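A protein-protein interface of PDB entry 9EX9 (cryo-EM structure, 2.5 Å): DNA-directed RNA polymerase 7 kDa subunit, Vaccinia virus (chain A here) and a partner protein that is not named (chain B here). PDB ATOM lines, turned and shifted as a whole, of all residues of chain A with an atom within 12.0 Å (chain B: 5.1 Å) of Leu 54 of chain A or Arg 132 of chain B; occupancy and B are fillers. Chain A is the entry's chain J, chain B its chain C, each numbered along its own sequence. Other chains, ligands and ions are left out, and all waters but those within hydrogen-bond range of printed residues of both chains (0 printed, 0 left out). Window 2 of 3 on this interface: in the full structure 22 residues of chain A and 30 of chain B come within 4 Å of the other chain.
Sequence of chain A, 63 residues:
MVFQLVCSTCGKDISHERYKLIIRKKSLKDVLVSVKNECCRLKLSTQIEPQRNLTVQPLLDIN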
ATOM      1  N   PRO A  50      -3.939   9.487  -9.116  1.00  0.00           N
ATOM      2  CA  PRO A  50      -3.807   8.214  -8.400  1.00  0.00           C
ATOM      3  C   PRO A  50      -5.009   7.304  -8.593  1.00  0.00           C
ATOM      4  O   PRO A  50      -6.114   7.745  -8.914  1.00  0.00           O
ATOM      5  CB  PRO A  50      -3.671   8.647  -6.937  1.00  0.00           C
ATOM      6  CG  PRO A  50      -4.340   9.959  -6.870  1.00  0.00           C
ATOM      7  CD  PRO A  50      -4.098  10.620  -8.190  1.00  0.00           C
ATOM      8  N   GLN A  51      -4.769   6.010  -8.402  1.00  0.00           N
ATOM      9  CA  GLN A  51      -5.818   5.003  -8.489  1.00  0.00           C
ATOM     10  C   GLN A  51      -6.632   4.995  -7.205  1.00  0.00           C
ATOM     11  O   GLN A  51      -6.069   4.940  -6.109  1.00  0.00           O
ATOM     12  CB  GLN A  51      -5.197   3.627  -8.729  1.00  0.00           C
ATOM     13  CG  GLN A  51      -6.196   2.501  -8.855  1.00  0.00           C
ATOM     14  CD  GLN A  51      -7.075   2.653 -10.070  1.00  0.00           C
ATOM     15  OE1 GLN A  51      -6.651   3.188 -11.093  1.00  0.00           O
ATOM     16  NE2 GLN A  51      -8.313   2.187  -9.965  1.00  0.00           N
ATOM     17  N   ARG A  52      -7.958   5.043  -7.334  1.00  0.00           N
ATOM     18  CA  ARG A  52      -8.818   5.122  -6.162  1.00  0.00           C
ATOM     19  C   ARG A  52     -10.146   4.431  -6.430  1.00  0.00           C
ATOM     20  O   ARG A  52     -10.621   4.381  -7.566  1.00  0.00           O
ATOM     21  CB  ARG A  52      -9.048   6.579  -5.752  1.00  0.00           C
ATOM     22  CG  ARG A  52      -7.800   7.232  -5.215  1.00  0.00           C
ATOM     23  CD  ARG A  52      -8.030   8.648  -4.797  1.00  0.00           C
ATOM     24  NE  ARG A  52      -6.841   9.195  -4.161  1.00  0.00           N
ATOM     25  CZ  ARG A  52      -6.716  10.451  -3.759  1.00  0.00           C
ATOM     26  NH1 ARG A  52      -7.689  11.330  -3.929  1.00  0.00           N
ATOM     27  NH2 ARG A  52      -5.589  10.834  -3.172  1.00  0.00           N
ATOM     28  N   ASN A  53     -10.740   3.900  -5.363  1.00  0.00           N
ATOM     29  CA  ASN A  53     -12.047   3.265  -5.421  1.00  0.00           C
ATOM     30  C   ASN A  53     -13.146   4.306  -5.257  1.00  0.00           C
ATOM     31  O   ASN A  53     -12.899   5.456  -4.895  1.00  0.00           O
ATOM     32  CB  ASN A  53     -12.181   2.204  -4.330  1.00  0.00           C
ATOM     33  CG  ASN A  53     -11.141   1.115  -4.434  1.00  0.00           C
ATOM     34  OD1 ASN A  53     -10.749   0.712  -5.525  1.00  0.00           O
ATOM     35  ND2 ASN A  53     -10.690   0.626  -3.288  1.00  0.00           N
ATOM     36  N   LEU A  54     -14.381   3.889  -5.516  1.00  0.00           N
ATOM     37  CA  LEU A  54     -15.521   4.748  -5.242  1.00  0.00           C
ATOM     38  C   LEU A  54     -15.706   4.908  -3.737  1.00  0.00           C
ATOM     39  O   LEU A  54     -15.222   4.100  -2.942  1.00  0.00           O
ATOM     40  CB  LEU A  54     -16.787   4.175  -5.869  1.00  0.00           C
ATOM     41  CG  LEU A  54     -16.734   3.951  -7.378  1.00  0.00           C
ATOM     42  CD1 LEU A  54     -18.038   3.376  -7.872  1.00  0.00           C
ATOM     43  CD2 LEU A  54     -16.429   5.237  -8.102  1.00  0.00           C
ATOM     44  N   THR A  55     -16.402   5.971  -3.345  1.00  0.00           N
ATOM     45  CA  THR A  55     -16.593   6.264  -1.931  1.00  0.00           C
ATOM     46  C   THR A  55     -17.853   5.585  -1.413  1.00  0.00           C
ATOM     47  O   THR A  55     -18.913   5.664  -2.039  1.00  0.00           O
ATOM     48  CB  THR A  55     -16.682   7.770  -1.694  1.00  0.00           C
ATOM     49  OG1 THR A  55     -17.928   8.263  -2.192  1.00  0.00           O
ATOM     50  CG2 THR A  55     -15.555   8.485  -2.394  1.00  0.00           C
ATOM     51  N   VAL A  56     -17.735   4.925  -0.270  1.00  0.00           N
ATOM     52  CA  VAL A  56     -18.871   4.256   0.349  1.00  0.00           C
ATOM     53  C   VAL A  56     -19.786   5.303   0.962  1.00  0.00           C
ATOM     54  O   VAL A  56     -19.337   6.164   1.726  1.00  0.00           O
ATOM     55  CB  VAL A  56     -18.395   3.253   1.410  1.00  0.00           C
ATOM     56  CG1 VAL A  56     -19.575   2.710   2.185  1.00  0.00           C
ATOM     57  CG2 VAL A  56     -17.613   2.131   0.759  1.00  0.00           C
ATOM     58  N   GLN A  57     -21.076   5.226   0.639  1.00  0.00           N
ATOM     59  CA  GLN A  57     -22.067   6.167   1.128  1.00  0.00           C
ATOM     60  C   GLN A  57     -23.150   5.429   1.905  1.00  0.00           C
ATOM     61  O   GLN A  57     -23.464   4.278   1.588  1.00  0.00           O
ATOM     62  CB  GLN A  57     -22.705   6.935  -0.034  1.00  0.00           C
ATOM     63  CG  GLN A  57     -21.698   7.672  -0.897  1.00  0.00           C
ATOM     64  CD  GLN A  57     -22.254   8.053  -2.248  1.00  0.00           C
ATOM     65  OE1 GLN A  57     -23.438   8.354  -2.382  1.00  0.00           O
ATOM     66  NE2 GLN A  57     -21.404   8.030  -3.263  1.00  0.00           N
ATOM     67  N   PRO A  58     -23.753   6.062   2.923  1.00  0.00           N
ATOM     68  CA  PRO A  58     -23.570   7.440   3.401  1.00  0.00           C
ATOM     69  C   PRO A  58     -22.276   7.645   4.169  1.00  0.00           C
ATOM     70  O   PRO A  58     -21.652   6.692   4.616  1.00  0.00           O
ATOM     71  CB  PRO A  58     -24.788   7.661   4.320  1.00  0.00           C
ATOM     72  CG  PRO A  58     -25.680   6.461   4.148  1.00  0.00           C
ATOM     73  CD  PRO A  58     -24.772   5.361   3.715  1.00  0.00           C
ATOM     74  N   LEU A  59     -21.853   8.897   4.325  1.00  0.00           N
ATOM     75  CA  LEU A  59     -20.657   9.194   5.101  1.00  0.00           C
ATOM     76  C   LEU A  59     -20.931   9.181   6.599  1.00  0.00           C
ATOM     77  O   LEU A  59     -20.000   9.020   7.393  1.00  0.00           O
ATOM     78  CB  LEU A  59     -20.087  10.545   4.672  1.00  0.00           C
ATOM     79  CG  LEU A  59     -19.528  10.574   3.248  1.00  0.00           C
ATOM     80  CD1 LEU A  59     -19.452  11.988   2.718  1.00  0.00           C
ATOM     81  CD2 LEU A  59     -18.160   9.932   3.211  1.00  0.00           C
ATOM     82  N   THR B  46     -13.989  10.920  -5.942  1.00  0.00           N
ATOM     83  CA  THR B  46     -12.901  10.130  -5.388  1.00  0.00           C
ATOM     84  C   THR B  46     -11.757  10.987  -4.867  1.00  0.00           C
ATOM     85  O   THR B  46     -10.685  10.452  -4.574  1.00  0.00           O
ATOM     86  CB  THR B  46     -12.374   9.148  -6.436  1.00  0.00           C
ATOM     87  OG1 THR B  46     -11.986   9.859  -7.614  1.00  0.00           O
ATOM     88  CG2 THR B  46     -13.438   8.136  -6.798  1.00  0.00           C
ATOM     89  N   GLN B  87     -20.947  12.684 -12.874  1.00  0.00           N
ATOM     90  CA  GLN B  87     -20.502  11.690 -13.836  1.00  0.00           C
ATOM     91  C   GLN B  87     -21.496  11.578 -14.986  1.00  0.00           C
ATOM     92  O   GLN B  87     -22.666  11.944 -14.871  1.00  0.00           O
ATOM     93  CB  GLN B  87     -20.335  10.334 -13.160  1.00  0.00           C
ATOM     94  CG  GLN B  87     -21.635   9.754 -12.653  1.00  0.00           C
ATOM     95  CD  GLN B  87     -21.427   8.542 -11.783  1.00  0.00           C
ATOM     96  OE1 GLN B  87     -20.306   8.070 -11.616  1.00  0.00           O
ATOM     97  NE2 GLN B  87     -22.509   8.031 -11.217  1.00  0.00           N
ATOM     98  N   GLN B 129     -14.175   8.266 -12.500  1.00  0.00           N
ATOM     99  CA  GLN B 129     -13.998   6.821 -12.560  1.00  0.00           C
ATOM    100  C   GLN B 129     -15.131   6.211 -13.385  1.00  0.00           C
ATOM    101  O   GLN B 129     -15.899   6.915 -14.047  1.00  0.00           O
ATOM    102  CB  GLN B 129     -13.934   6.240 -11.152  1.00  0.00           C
ATOM    103  CG  GLN B 129     -12.787   6.775 -10.319  1.00  0.00           C
ATOM    104  CD  GLN B 129     -11.428   6.373 -10.860  1.00  0.00           C
ATOM    105  OE1 GLN B 129     -11.330   5.604 -11.815  1.00  0.00           O
ATOM    106  NE2 GLN B 129     -10.370   6.892 -10.248  1.00  0.00           N
ATOM    107  N   GLU B 130     -15.251   4.887 -13.355  1.00  0.00           N
ATOM    108  CA  GLU B 130     -16.249   4.213 -14.175  1.00  0.00           C
ATOM    109  C   GLU B 130     -17.655   4.659 -13.797  1.00  0.00           C
ATOM    110  O   GLU B 130     -17.970   4.857 -12.623  1.00  0.00           O
ATOM    111  CB  GLU B 130     -16.129   2.699 -14.026  1.00  0.00           C
ATOM    112  CG  GLU B 130     -14.876   2.107 -14.650  1.00  0.00           C
ATOM    113  CD  GLU B 130     -14.931   0.592 -14.735  1.00  0.00           C
ATOM    114  OE1 GLU B 130     -16.002   0.016 -14.451  1.00  0.00           O
ATOM    115  OE2 GLU B 130     -13.902  -0.024 -15.086  1.00  0.00           O
ATOM    116  N   TYR B 131     -18.506   4.795 -14.808  1.00  0.00           N
ATOM    117  CA  TYR B 131     -19.861   5.292 -14.620  1.00  0.00           C
ATOM    118  C   TYR B 131     -20.767   4.179 -14.103  1.00  0.00           C
ATOM    119  O   TYR B 131     -21.004   3.189 -14.802  1.00  0.00           O
ATOM    120  CB  TYR B 131     -20.382   5.847 -15.942  1.00  0.00           C
ATOM    121  CG  TYR B 131     -21.833   6.256 -15.930  1.00  0.00           C
ATOM    122  CD1 TYR B 131     -22.240   7.418 -15.304  1.00  0.00           C
ATOM    123  CD2 TYR B 131     -22.790   5.489 -16.568  1.00  0.00           C
ATOM    124  CE1 TYR B 131     -23.561   7.798 -15.301  1.00  0.00           C
ATOM    125  CE2 TYR B 131     -24.113   5.862 -16.571  1.00  0.00           C
ATOM    126  CZ  TYR B 131     -24.493   7.018 -15.936  1.00  0.00           C
ATOM    127  OH  TYR B 131     -25.815   7.395 -15.936  1.00  0.00           O
ATOM    128  N   ARG B 132     -21.274   4.343 -12.883  1.00  0.00           N
ATOM    129  CA  ARG B 132     -22.266   3.447 -12.299  1.00  0.00           C
ATOM    130  C   ARG B 132     -23.547   4.232 -12.069  1.00  0.00           C
ATOM    131  O   ARG B 132     -23.539   5.241 -11.358  1.00  0.00           O
ATOM    132  CB  ARG B 132     -21.781   2.851 -10.979  1.00  0.00           C
ATOM    133  CG  ARG B 132     -20.746   1.764 -11.118  1.00  0.00           C
ATOM    134  CD  ARG B 132     -20.495   1.103  -9.778  1.00  0.00           C
ATOM    135  NE  ARG B 132     -19.368   0.180  -9.819  1.00  0.00           N
ATOM    136  CZ  ARG B 132     -18.853  -0.420  -8.754  1.00  0.00           C
ATOM    137  NH1 ARG B 132     -19.345  -0.219  -7.543  1.00  0.00           N
ATOM    138  NH2 ARG B 132     -17.815  -1.236  -8.908  1.00  0.00           N
ATOM    139  N   LEU B 133     -24.645   3.761 -12.654  1.00  0.00           N
ATOM    140  CA  LEU B 133     -25.909   4.472 -12.509  1.00  0.00           C
ATOM    141  C   LEU B 133     -26.411   4.424 -11.072  1.00  0.00           C
ATOM    142  O   LEU B 133     -27.020   5.386 -10.590  1.00  0.00           O
ATOM    143  CB  LEU B 133     -26.949   3.888 -13.459  1.00  0.00           C
ATOM    144  CG  LEU B 133     -28.340   4.516 -13.365  1.00  0.00           C
ATOM    145  CD1 LEU B 133     -28.270   6.023 -13.557  1.00  0.00           C
ATOM    146  CD2 LEU B 133     -29.274   3.889 -14.383  1.00  0.00           C
ATOM    147  N   LYS B 134     -26.175   3.314 -10.373  1.00  0.00           N
ATOM    148  CA  LYS B 134     -26.705   3.166  -9.022  1.00  0.00           C
ATOM    149  C   LYS B 134     -26.103   4.197  -8.075  1.00  0.00           C
ATOM    150  O   LYS B 134     -26.824   4.861  -7.321  1.00  0.00           O
ATOM    151  CB  LYS B 134     -26.437   1.752  -8.508  1.00  0.00           C
ATOM    152  CG  LYS B 134     -27.118   0.667  -9.318  1.00  0.00           C
ATOM    153  CD  LYS B 134     -26.795  -0.716  -8.781  1.00  0.00           C
ATOM    154  CE  LYS B 134     -27.459  -1.799  -9.614  1.00  0.00           C
ATOM    155  NZ  LYS B 134     -27.088  -3.163  -9.152  1.00  0.00           N
ATOM    156  N   SER B 135     -24.786   4.350  -8.104  1.00  0.00           N
ATOM    157  CA  SER B 135     -24.094   5.210  -7.159  1.00  0.00           C
ATOM    158  C   SER B 135     -24.085   6.654  -7.653  1.00  0.00           C
ATOM    159  O   SER B 135     -24.491   6.960  -8.774  1.00  0.00           O
ATOM    160  CB  SER B 135     -22.667   4.711  -6.938  1.00  0.00           C
ATOM    161  OG  SER B 135     -22.046   5.398  -5.868  1.00  0.00           O
ATOM    162  N   GLN B 137     -21.722  10.263  -8.059  1.00  0.00           N
ATOM    163  CA  GLN B 137     -20.363  10.785  -8.175  1.00  0.00           C
ATOM    164  C   GLN B 137     -20.486  12.209  -8.708  1.00  0.00           C
ATOM    165  O   GLN B 137     -20.596  12.409  -9.920  1.00  0.00           O
ATOM    166  CB  GLN B 137     -19.519   9.910  -9.087  1.00  0.00           C
ATOM    167  CG  GLN B 137     -18.032  10.012  -8.849  1.00  0.00           C
ATOM    168  CD  GLN B 137     -17.245   9.067  -9.727  1.00  0.00           C
ATOM    169  OE1 GLN B 137     -17.784   8.475 -10.658  1.00  0.00           O
ATOM    170  NE2 GLN B 137     -15.965   8.919  -9.432  1.00  0.00           N
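The side-chain amide nitrogen of Gln 87 of chain B sits at hydrogen-bond distance from the backbone carbonyl oxygen of Arg 132 of chain B (3.0 Å).
O of Ser 135 of chain B lies within hydrogen-bond range of NE2 of Gln 87 of chain B (3.3 Å).
OE1 of Gln 87 of chain B lies close to OE1 of Gln 137 of chain B.
Of the 10 printed residues of chain A, 4 touch a printed residue of chain B.
Among the printed residues, 6 pairs touch across the chains.
Among the printed residues, no Asp or Glu carboxylate lies within 4 Å of a Lys or Arg side-chain nitrogen of the other chain.
Of the printed residues of chain B, Arg 52 of chain A touches Thr 46 (3.2 Å) and Gln 129 (3.7 Å).
Leu 54 of chain A touches just these residues of chain B: Arg 132 (3.8 Å) and Gln 137 (3.9 Å).
Of the printed residues of chain B, Gln 57 of chain A touches Ser 135 (3.8 Å).
Printed residues of chain A within 4 Å of Thr 46 of chain B: Arg 52 and Asn 53.
No residue of chain A comes within 4 Å of Glu 130 of chain B.
Arg 132 of chain B touches just one residue of chain A: Leu 54 (3.8 Å).
No residue of chain A comes within 4 Å of Leu 133 of chain B.
No residue of chain A comes within 4 Å of Lys 134 of chain B.
Ser 135 of chain B touches just one residue of chain A: Gln 57 (3.8 Å).
Printed residues of chain A within 4 Å of Gln 137 of chain B: Leu 54 (3.9 Å).
The nearest residue of chain B that does not touch Leu 54 of chain A is Gln 129 of chain B (4.1 Å).
NH1 of Arg 52 of chain A lies within hydrogen-bond range of O of Thr 46 of chain B (3.2 Å).
Gln 129 of chain B touches Arg 52 of chain A (NE2 to O, 3.7 Å).
Asn 53 of chain A touches Thr 46 of chain B.
Leu 54 of chain A touches Arg 132 of chain B.
CD2 of Leu 54 of chain A touches NE2 of Gln 137 of chain B (3.9 Å).
Gln 57 of chain A touches Ser 135 of chain B.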
